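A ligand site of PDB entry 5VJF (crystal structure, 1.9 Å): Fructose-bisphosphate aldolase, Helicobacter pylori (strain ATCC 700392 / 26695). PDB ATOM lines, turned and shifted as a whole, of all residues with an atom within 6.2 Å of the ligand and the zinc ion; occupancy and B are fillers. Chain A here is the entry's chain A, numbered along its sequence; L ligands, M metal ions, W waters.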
ATOM      1  N   ALA A  21     -22.957  -4.651  -9.855  1.00  0.00           N
ATOM      2  CA  ALA A  21     -21.540  -4.968  -9.918  1.00  0.00           C
ATOM      3  C   ALA A  21     -21.294  -6.103  -8.928  1.00  0.00           C
ATOM      4  O   ALA A  21     -21.360  -5.926  -7.714  1.00  0.00           O
ATOM      5  CB  ALA A  21     -20.707  -3.768  -9.567  1.00  0.00           C
ATOM      6  N   ASN A  23     -19.311  -9.267  -7.241  1.00  0.00           N
ATOM      7  CA  ASN A  23     -17.990  -9.784  -6.920  1.00  0.00           C
ATOM      8  C   ASN A  23     -17.898 -11.282  -7.218  1.00  0.00           C
ATOM      9  O   ASN A  23     -18.893 -11.994  -7.076  1.00  0.00           O
ATOM     10  CB  ASN A  23     -17.642  -9.533  -5.447  1.00  0.00           C
ATOM     11  CG  ASN A  23     -17.346  -8.071  -5.170  1.00  0.00           C
ATOM     12  OD1 ASN A  23     -18.251  -7.263  -5.055  1.00  0.00           O
ATOM     13  ND2 ASN A  23     -16.071  -7.737  -5.057  1.00  0.00           N
ATOM     14  N   GLN A  47     -16.693  -7.811 -10.740  1.00  0.00           N
ATOM     15  CA  GLN A  47     -15.609  -7.183  -9.986  1.00  0.00           C
ATOM     16  C   GLN A  47     -14.873  -8.137  -9.072  1.00  0.00           C
ATOM     17  O   GLN A  47     -15.404  -9.157  -8.626  1.00  0.00           O
ATOM     18  CB  GLN A  47     -16.081  -5.917  -9.256  1.00  0.00           C
ATOM     19  CG  GLN A  47     -17.287  -6.040  -8.370  1.00  0.00           C
ATOM     20  CD  GLN A  47     -17.628  -4.712  -7.682  1.00  0.00           C
ATOM     21  OE1 GLN A  47     -17.517  -3.646  -8.284  1.00  0.00           O
ATOM     22  NE2 GLN A  47     -18.043  -4.792  -6.432  1.00  0.00           N
ATOM     23  N   ASP A  82     -12.202  -3.918  -7.579  1.00  0.00           N
ATOM     24  CA  ASP A  82     -12.947  -3.406  -6.435  1.00  0.00           C
ATOM     25  C   ASP A  82     -11.985  -3.078  -5.299  1.00  0.00           C
ATOM     26  O   ASP A  82     -11.117  -3.879  -4.958  1.00  0.00           O
ATOM     27  CB  ASP A  82     -13.977  -4.443  -5.984  1.00  0.00           C
ATOM     28  CG  ASP A  82     -14.936  -3.921  -4.931  1.00  0.00           C
ATOM     29  OD1 ASP A  82     -15.200  -2.694  -4.868  1.00  0.00           O
ATOM     30  OD2 ASP A  82     -15.444  -4.763  -4.147  1.00  0.00           O
ATOM     31  N   HIS A  83     -12.135  -1.875  -4.740  1.00  0.00           N
ATOM     32  CA  HIS A  83     -11.284  -1.399  -3.652  1.00  0.00           C
ATOM     33  C   HIS A  83      -9.783  -1.582  -3.870  1.00  0.00           C
ATOM     34  O   HIS A  83      -9.091  -2.202  -3.052  1.00  0.00           O
ATOM     35  CB  HIS A  83     -11.728  -2.033  -2.332  1.00  0.00           C
ATOM     36  CG  HIS A  83     -12.986  -1.449  -1.794  1.00  0.00           C
ATOM     37  ND1 HIS A  83     -13.007  -0.284  -1.066  1.00  0.00           N
ATOM     38  CD2 HIS A  83     -14.270  -1.850  -1.901  1.00  0.00           C
ATOM     39  CE1 HIS A  83     -14.260   0.007  -0.731  1.00  0.00           C
ATOM     40  NE2 HIS A  83     -15.046  -0.931  -1.231  1.00  0.00           N
ATOM     41  N   MET A 102     -11.177   0.753  -9.260  1.00  0.00           N
ATOM     42  CA  MET A 102     -11.495   1.658  -8.167  1.00  0.00           C
ATOM     43  C   MET A 102     -10.243   1.927  -7.358  1.00  0.00           C
ATOM     44  O   MET A 102      -9.566   0.998  -6.936  1.00  0.00           O
ATOM     45  CB  MET A 102     -12.548   1.061  -7.243  1.00  0.00           C
ATOM     46  CG  MET A 102     -12.925   2.017  -6.111  1.00  0.00           C
ATOM     47  SD  MET A 102     -13.612   1.213  -4.670  1.00  0.00           S
ATOM     48  CE  MET A 102     -14.108   2.614  -3.678  1.00  0.00           C
ATOM     49  N   ASP A 104      -9.474   3.399  -3.832  1.00  0.00           N
ATOM     50  CA  ASP A 104     -10.143   3.788  -2.601  1.00  0.00           C
ATOM     51  C   ASP A 104      -9.171   4.452  -1.641  1.00  0.00           C
ATOM     52  O   ASP A 104      -8.372   3.791  -0.974  1.00  0.00           O
ATOM     53  CB  ASP A 104     -10.797   2.575  -1.936  1.00  0.00           C
ATOM     54  CG  ASP A 104     -11.519   2.930  -0.663  1.00  0.00           C
ATOM     55  OD1 ASP A 104     -11.691   4.135  -0.362  1.00  0.00           O
ATOM     56  OD2 ASP A 104     -11.930   1.994   0.040  1.00  0.00           O
ATOM     57  N   GLU A 134     -13.887   7.099  -4.108  1.00  0.00           N
ATOM     58  CA  GLU A 134     -14.847   7.092  -3.019  1.00  0.00           C
ATOM     59  C   GLU A 134     -14.667   8.325  -2.143  1.00  0.00           C
ATOM     60  O   GLU A 134     -13.547   8.782  -1.907  1.00  0.00           O
ATOM     61  CB  GLU A 134     -14.728   5.806  -2.197  1.00  0.00           C
ATOM     62  CG  GLU A 134     -15.748   5.688  -1.063  1.00  0.00           C
ATOM     63  CD  GLU A 134     -15.816   4.269  -0.491  1.00  0.00           C
ATOM     64  OE1 GLU A 134     -14.796   3.780   0.033  1.00  0.00           O
ATOM     65  OE2 GLU A 134     -16.897   3.638  -0.561  1.00  0.00           O
ATOM     66  N   LEU A 138     -17.762   4.714   5.022  1.00  0.00           N
ATOM     67  CA  LEU A 138     -18.708   3.679   5.420  1.00  0.00           C
ATOM     68  C   LEU A 138     -18.302   3.106   6.774  1.00  0.00           C
ATOM     69  O   LEU A 138     -17.191   2.598   6.934  1.00  0.00           O
ATOM     70  CB  LEU A 138     -18.759   2.564   4.369  1.00  0.00           C
ATOM     71  CG  LEU A 138     -19.699   2.775   3.178  1.00  0.00           C
ATOM     72  CD1 LEU A 138     -19.455   4.097   2.480  1.00  0.00           C
ATOM     73  CD2 LEU A 138     -19.583   1.612   2.205  1.00  0.00           C
ATOM     74  N   SER A 179     -23.019   0.252   4.448  1.00  0.00           N
ATOM     75  CA  SER A 179     -21.714  -0.283   4.824  1.00  0.00           C
ATOM     76  C   SER A 179     -21.609  -1.695   4.294  1.00  0.00           C
ATOM     77  O   SER A 179     -22.617  -2.294   3.930  1.00  0.00           O
ATOM     78  CB  SER A 179     -21.533  -0.273   6.347  1.00  0.00           C
ATOM     79  OG  SER A 179     -22.650  -0.860   6.983  1.00  0.00           O
ATOM     80  N   HIS A 180     -20.397  -2.231   4.246  1.00  0.00           N
ATOM     81  CA  HIS A 180     -20.180  -3.568   3.729  1.00  0.00           C
ATOM     82  C   HIS A 180     -20.713  -4.604   4.698  1.00  0.00           C
ATOM     83  O   HIS A 180     -20.744  -4.374   5.903  1.00  0.00           O
ATOM     84  CB  HIS A 180     -18.690  -3.831   3.522  1.00  0.00           C
ATOM     85  CG  HIS A 180     -18.122  -3.177   2.307  1.00  0.00           C
ATOM     86  ND1 HIS A 180     -17.349  -3.862   1.394  1.00  0.00           N
ATOM     87  CD2 HIS A 180     -18.219  -1.911   1.854  1.00  0.00           C
ATOM     88  CE1 HIS A 180     -16.985  -3.024   0.430  1.00  0.00           C
ATOM     89  NE2 HIS A 180     -17.503  -1.839   0.681  1.00  0.00           N
ATOM     90  N   GLY A 181     -21.106  -5.755   4.172  1.00  0.00           N
ATOM     91  CA  GLY A 181     -21.446  -6.880   5.003  1.00  0.00           C
ATOM     92  C   GLY A 181     -22.921  -7.016   5.326  1.00  0.00           C
ATOM     93  O   GLY A 181     -23.773  -6.287   4.836  1.00  0.00           O
ATOM     94  N   ALA A 182     -23.207  -7.972   6.201  1.00  0.00           N
ATOM     95  CA  ALA A 182     -24.554  -8.421   6.457  1.00  0.00           C
ATOM     96  C   ALA A 182     -25.228  -7.661   7.601  1.00  0.00           C
ATOM     97  O   ALA A 182     -26.403  -7.890   7.885  1.00  0.00           O
ATOM     98  CB  ALA A 182     -24.531  -9.901   6.780  1.00  0.00           C
ATOM     99  N   LYS A 184     -25.837  -4.082   8.361  1.00  0.00           N
ATOM    100  CA  LYS A 184     -25.755  -2.704   7.874  1.00  0.00           C
ATOM    101  C   LYS A 184     -26.432  -1.665   8.769  1.00  0.00           C
ATOM    102  O   LYS A 184     -26.017  -0.507   8.779  1.00  0.00           O
ATOM    103  CB  LYS A 184     -26.347  -2.614   6.469  1.00  0.00           C
ATOM    104  CG  LYS A 184     -25.684  -3.540   5.457  1.00  0.00           C
ATOM    105  CD  LYS A 184     -26.163  -3.264   4.048  1.00  0.00           C
ATOM    106  CE  LYS A 184     -25.647  -4.328   3.076  1.00  0.00           C
ATOM    107  NZ  LYS A 184     -24.155  -4.374   3.047  1.00  0.00           N
ATOM    108  N   LEU A 209     -23.047   2.782  -5.533  1.00  0.00           N
ATOM    109  CA  LEU A 209     -23.462   2.442  -4.181  1.00  0.00           C
ATOM    110  C   LEU A 209     -22.695   1.220  -3.696  1.00  0.00           C
ATOM    111  O   LEU A 209     -22.847   0.124  -4.235  1.00  0.00           O
ATOM    112  CB  LEU A 209     -24.952   2.126  -4.147  1.00  0.00           C
ATOM    113  CG  LEU A 209     -25.560   1.934  -2.753  1.00  0.00           C
ATOM    114  CD1 LEU A 209     -25.475   3.244  -1.966  1.00  0.00           C
ATOM    115  CD2 LEU A 209     -26.992   1.476  -2.850  1.00  0.00           C
ATOM    116  N   HIS A 210     -21.857   1.423  -2.671  1.00  0.00           N
ATOM    117  CA  HIS A 210     -21.204   0.296  -2.005  1.00  0.00           C
ATOM    118  C   HIS A 210     -22.098  -0.242  -0.897  1.00  0.00           C
ATOM    119  O   HIS A 210     -23.022   0.440  -0.450  1.00  0.00           O
ATOM    120  CB  HIS A 210     -19.837   0.702  -1.454  1.00  0.00           C
ATOM    121  CG  HIS A 210     -18.787   0.877  -2.504  1.00  0.00           C
ATOM    122  ND1 HIS A 210     -17.604   0.182  -2.496  1.00  0.00           N
ATOM    123  CD2 HIS A 210     -18.766   1.639  -3.620  1.00  0.00           C
ATOM    124  CE1 HIS A 210     -16.886   0.527  -3.542  1.00  0.00           C
ATOM    125  NE2 HIS A 210     -17.561   1.414  -4.238  1.00  0.00           N
ATOM    126  N   GLY A 211     -21.807  -1.467  -0.474  1.00  0.00           N
ATOM    127  CA  GLY A 211     -22.551  -2.111   0.599  1.00  0.00           C
ATOM    128  C   GLY A 211     -24.024  -2.247   0.297  1.00  0.00           C
ATOM    129  O   GLY A 211     -24.859  -1.974   1.152  1.00  0.00           O
ATOM    130  N   ALA A 212     -24.331  -2.673  -0.927  1.00  0.00           N
ATOM    131  CA  ALA A 212     -25.703  -2.621  -1.449  1.00  0.00           C
ATOM    132  C   ALA A 212     -26.454  -3.955  -1.398  1.00  0.00           C
ATOM    133  O   ALA A 212     -27.525  -4.060  -1.995  1.00  0.00           O
ATOM    134  CB  ALA A 212     -25.692  -2.084  -2.880  1.00  0.00           C
ATOM    135  N   SER A 213     -25.915  -4.955  -0.706  1.00  0.00           N
ATOM    136  CA  SER A 213     -26.625  -6.222  -0.550  1.00  0.00           C
ATOM    137  C   SER A 213     -27.911  -6.010   0.246  1.00  0.00           C
ATOM    138  O   SER A 213     -27.977  -5.161   1.126  1.00  0.00           O
ATOM    139  CB  SER A 213     -25.732  -7.267   0.124  1.00  0.00           C
ATOM    140  OG  SER A 213     -24.866  -7.868  -0.829  1.00  0.00           O
ATOM    141  N   ALA A 214     -28.948  -6.785  -0.081  1.00  0.00           N
ATOM    142  CA  ALA A 214     -30.258  -6.624   0.531  1.00  0.00           C
ATOM    143  C   ALA A 214     -30.557  -7.687   1.596  1.00  0.00           C
ATOM    144  O   ALA A 214     -31.416  -7.475   2.463  1.00  0.00           O
ATOM    145  CB  ALA A 214     -31.329  -6.685  -0.545  1.00  0.00           C
ATOM    146  N   LYS A 251     -24.173   2.188 -10.485  1.00  0.00           N
ATOM    147  CA  LYS A 251     -23.415   0.948 -10.259  1.00  0.00           C
ATOM    148  C   LYS A 251     -23.683   0.481  -8.823  1.00  0.00           C
ATOM    149  O   LYS A 251     -23.533   1.251  -7.867  1.00  0.00           O
ATOM    150  CB  LYS A 251     -21.920   1.190 -10.484  1.00  0.00           C
ATOM    151  CG  LYS A 251     -21.005  -0.006 -10.175  1.00  0.00           C
ATOM    152  CD  LYS A 251     -19.548   0.328 -10.538  1.00  0.00           C
ATOM    153  CE  LYS A 251     -18.563  -0.782 -10.137  1.00  0.00           C
ATOM    154  NZ  LYS A 251     -18.229  -0.761  -8.689  1.00  0.00           N
ATOM    155  N   ASN A 253     -22.946  -2.264  -6.017  1.00  0.00           N
ATOM    156  CA  ASN A 253     -22.010  -3.294  -5.599  1.00  0.00           C
ATOM    157  C   ASN A 253     -22.672  -4.337  -4.708  1.00  0.00           C
ATOM    158  O   ASN A 253     -23.277  -4.013  -3.695  1.00  0.00           O
ATOM    159  CB  ASN A 253     -20.833  -2.677  -4.849  1.00  0.00           C
ATOM    160  CG  ASN A 253     -19.907  -1.868  -5.756  1.00  0.00           C
ATOM    161  OD1 ASN A 253     -20.272  -1.470  -6.861  1.00  0.00           O
ATOM    162  ND2 ASN A 253     -18.685  -1.652  -5.289  1.00  0.00           N
ATOM    163  N   THR A 254     -22.522  -5.593  -5.110  1.00  0.00           N
ATOM    164  CA  THR A 254     -23.256  -6.697  -4.479  1.00  0.00           C
ATOM    165  C   THR A 254     -22.354  -7.908  -4.359  1.00  0.00           C
ATOM    166  O   THR A 254     -21.865  -8.420  -5.360  1.00  0.00           O
ATOM    167  CB  THR A 254     -24.475  -7.073  -5.336  1.00  0.00           C
ATOM    168  OG1 THR A 254     -25.217  -5.896  -5.671  1.00  0.00           O
ATOM    169  CG2 THR A 254     -25.373  -8.055  -4.586  1.00  0.00           C
ATOM    170  N   ASP A 255     -22.141  -8.363  -3.128  1.00  0.00           N
ATOM    171  CA  ASP A 255     -21.230  -9.468  -2.845  1.00  0.00           C
ATOM    172  C   ASP A 255     -21.829 -10.365  -1.773  1.00  0.00           C
ATOM    173  O   ASP A 255     -21.986 -11.566  -1.965  1.00  0.00           O
ATOM    174  CB  ASP A 255     -19.888  -8.885  -2.380  1.00  0.00           C
ATOM    175  CG  ASP A 255     -18.799  -9.947  -2.228  1.00  0.00           C
ATOM    176  OD1 ASP A 255     -19.085 -11.146  -2.413  1.00  0.00           O
ATOM    177  OD2 ASP A 255     -17.641  -9.568  -1.944  1.00  0.00           O
ATOM    178  N   THR A 256     -22.190  -9.766  -0.640  1.00  0.00           N
ATOM    179  CA  THR A 256     -22.725 -10.537   0.488  1.00  0.00           C
ATOM    180  C   THR A 256     -23.940 -11.400   0.145  1.00  0.00           C
ATOM    181  O   THR A 256     -24.000 -12.579   0.541  1.00  0.00           O
ATOM    182  CB  THR A 256     -23.033  -9.594   1.684  1.00  0.00           C
ATOM    183  OG1 THR A 256     -21.807  -8.995   2.109  1.00  0.00           O
ATOM    184  CG2 THR A 256     -23.624 -10.346   2.850  1.00  0.00           C
ATOM    185  N   ASP A 257     -24.892 -10.862  -0.621  1.00  0.00           N
ATOM    186  CA  ASP A 257     -26.065 -11.651  -1.009  1.00  0.00           C
ATOM    187  C   ASP A 257     -25.642 -12.896  -1.779  1.00  0.00           C
ATOM    188  O   ASP A 257     -26.209 -13.979  -1.599  1.00  0.00           O
ATOM    189  CB  ASP A 257     -26.996 -10.842  -1.898  1.00  0.00           C
ATOM    190  CG  ASP A 257     -27.809  -9.831  -1.129  1.00  0.00           C
ATOM    191  OD1 ASP A 257     -27.842  -9.902   0.126  1.00  0.00           O
ATOM    192  OD2 ASP A 257     -28.438  -8.972  -1.801  1.00  0.00           O
HETATM  193  P1  LIG L   1     -22.086  -5.879   0.226  1.00  0.00           P
HETATM  194  O1  LIG L   1     -23.451  -5.095   0.681  1.00  0.00           O
HETATM  195  O2  LIG L   1     -21.294  -6.473   1.540  1.00  0.00           O
HETATM  196  O3  LIG L   1     -22.433  -6.983  -0.672  1.00  0.00           O
HETATM  197  O4  LIG L   1     -21.089  -4.799  -0.531  1.00  0.00           O
HETATM  198  C1  LIG L   1     -20.448  -5.082  -1.747  1.00  0.00           C
HETATM  199  C2  LIG L   1     -19.398  -3.996  -2.050  1.00  0.00           C
HETATM  200  O5  LIG L   1     -19.586  -2.846  -1.755  1.00  0.00           O
HETATM  201  C3  LIG L   1     -18.113  -4.403  -2.792  1.00  0.00           C
HETATM  202  O6  LIG L   1     -17.405  -3.248  -3.121  1.00  0.00           O
HETATM  203 ZN    ZN M   1     -16.989  -0.879  -0.929  1.00  0.00          ZN
HETATM  204  O   HOH W   1     -16.729   1.369   0.526  1.00  0.00           O
HETATM  205  O   HOH W   2     -18.613  -7.186   1.225  1.00  0.00           O
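The zinc ion is bound by a ring nitrogen (NE2) of His 180 (1.9 Å), a ring nitrogen (NE2) of His 83 (2.0 Å) and a ring nitrogen (ND1) of His 210 (2.0 Å). The zinc ion has three donor atoms within binding distance. Slightly farther from the zinc ion lies water W1 (2.7 Å).
Residues that only touch the ligand: Asn 23 (3.6 Å), Gln 47 (3.7 Å) and Thr 254 (3.8 Å). Hydrophobic or aromatic side chains within 4 Å of the ligand: His 83, His 180 and His 210. Of the 26 residues printed, 15 come within 4 Å of the ligand. The nearest printed residue that does not touch the ligand is Ser 179 (4.4 Å).
N of His 83 lies within hydrogen-bond range of SD of Met 102 (3.4 Å). OD2 of Asp 104 sits close to ND1 of His 83, at 2.8 Å. ND2 of Asn 253 sits close to NE2 of His 210 (3.4 Å). The side-chain amino group of Lys 184 is in hydrogen-bond range of the backbone carbonyl oxygen of Gly 211. OD2 of Asp 82 lies within hydrogen-bond range of NE2 of Gln 47. The backbone NH of Asn 23 is in hydrogen-bond range of the backbone carbonyl oxygen of Thr 254 (3.3 Å). The side-chain amino group (NZ) of Lys 251 sits at hydrogen-bond distance from the side-chain amide oxygen (OE1) of Gln 47 (3.0 Å). The backbone NH (N) of Thr 254 lies within hydrogen-bond range of the backbone carbonyl oxygen (O) of Ala 21 (2.9 Å).
A ring nitrogen (NE2) of His 180 lies close to an oxygen (O5) of the ligand (3.4 Å). A ring nitrogen (ND1) of His 210 lies close to an oxygen (O6) of the ligand (3.5 Å). NZ of Lys 184 is in salt-bridge range of O1 of the ligand. The backbone NH (N) of Ser 213 sits at hydrogen-bond distance from an oxygen (O1) of the ligand, at 2.8 Å. The side-chain hydroxyl (OG) of Ser 213 is in hydrogen-bond range of an oxygen (O3) of the ligand (2.6 Å). The backbone NH (N) of Thr 256 is in hydrogen-bond range of an oxygen (O3) of the ligand, at 2.8 Å. An oxygen (O2) of the ligand is in hydrogen-bond range of the side-chain hydroxyl (OG1) of Thr 256, at 2.6 Å. An oxygen (O6) of the ligand lies within hydrogen-bond range of the side-chain carboxylate (OD2) of Asp 82. The backbone NH (N) of Gly 181 lies within hydrogen-bond range of an oxygen (O2) of the ligand, 2.7 Å away. An oxygen (O3) of the ligand lies within hydrogen-bond range of the backbone NH (N) of Asp 255, 2.8 Å away. O5 of the ligand lies within hydrogen-bond range of N of Gly 211. ND2 of Asn 253 sits at hydrogen-bond distance from O6 of the ligand (3.0 Å). The backbone NH (N) of Ala 212 sits at hydrogen-bond distance from an oxygen (O1) of the ligand (3.0 Å).
Within 4 Å of the zinc ion: His 83, His 180 and His 210.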
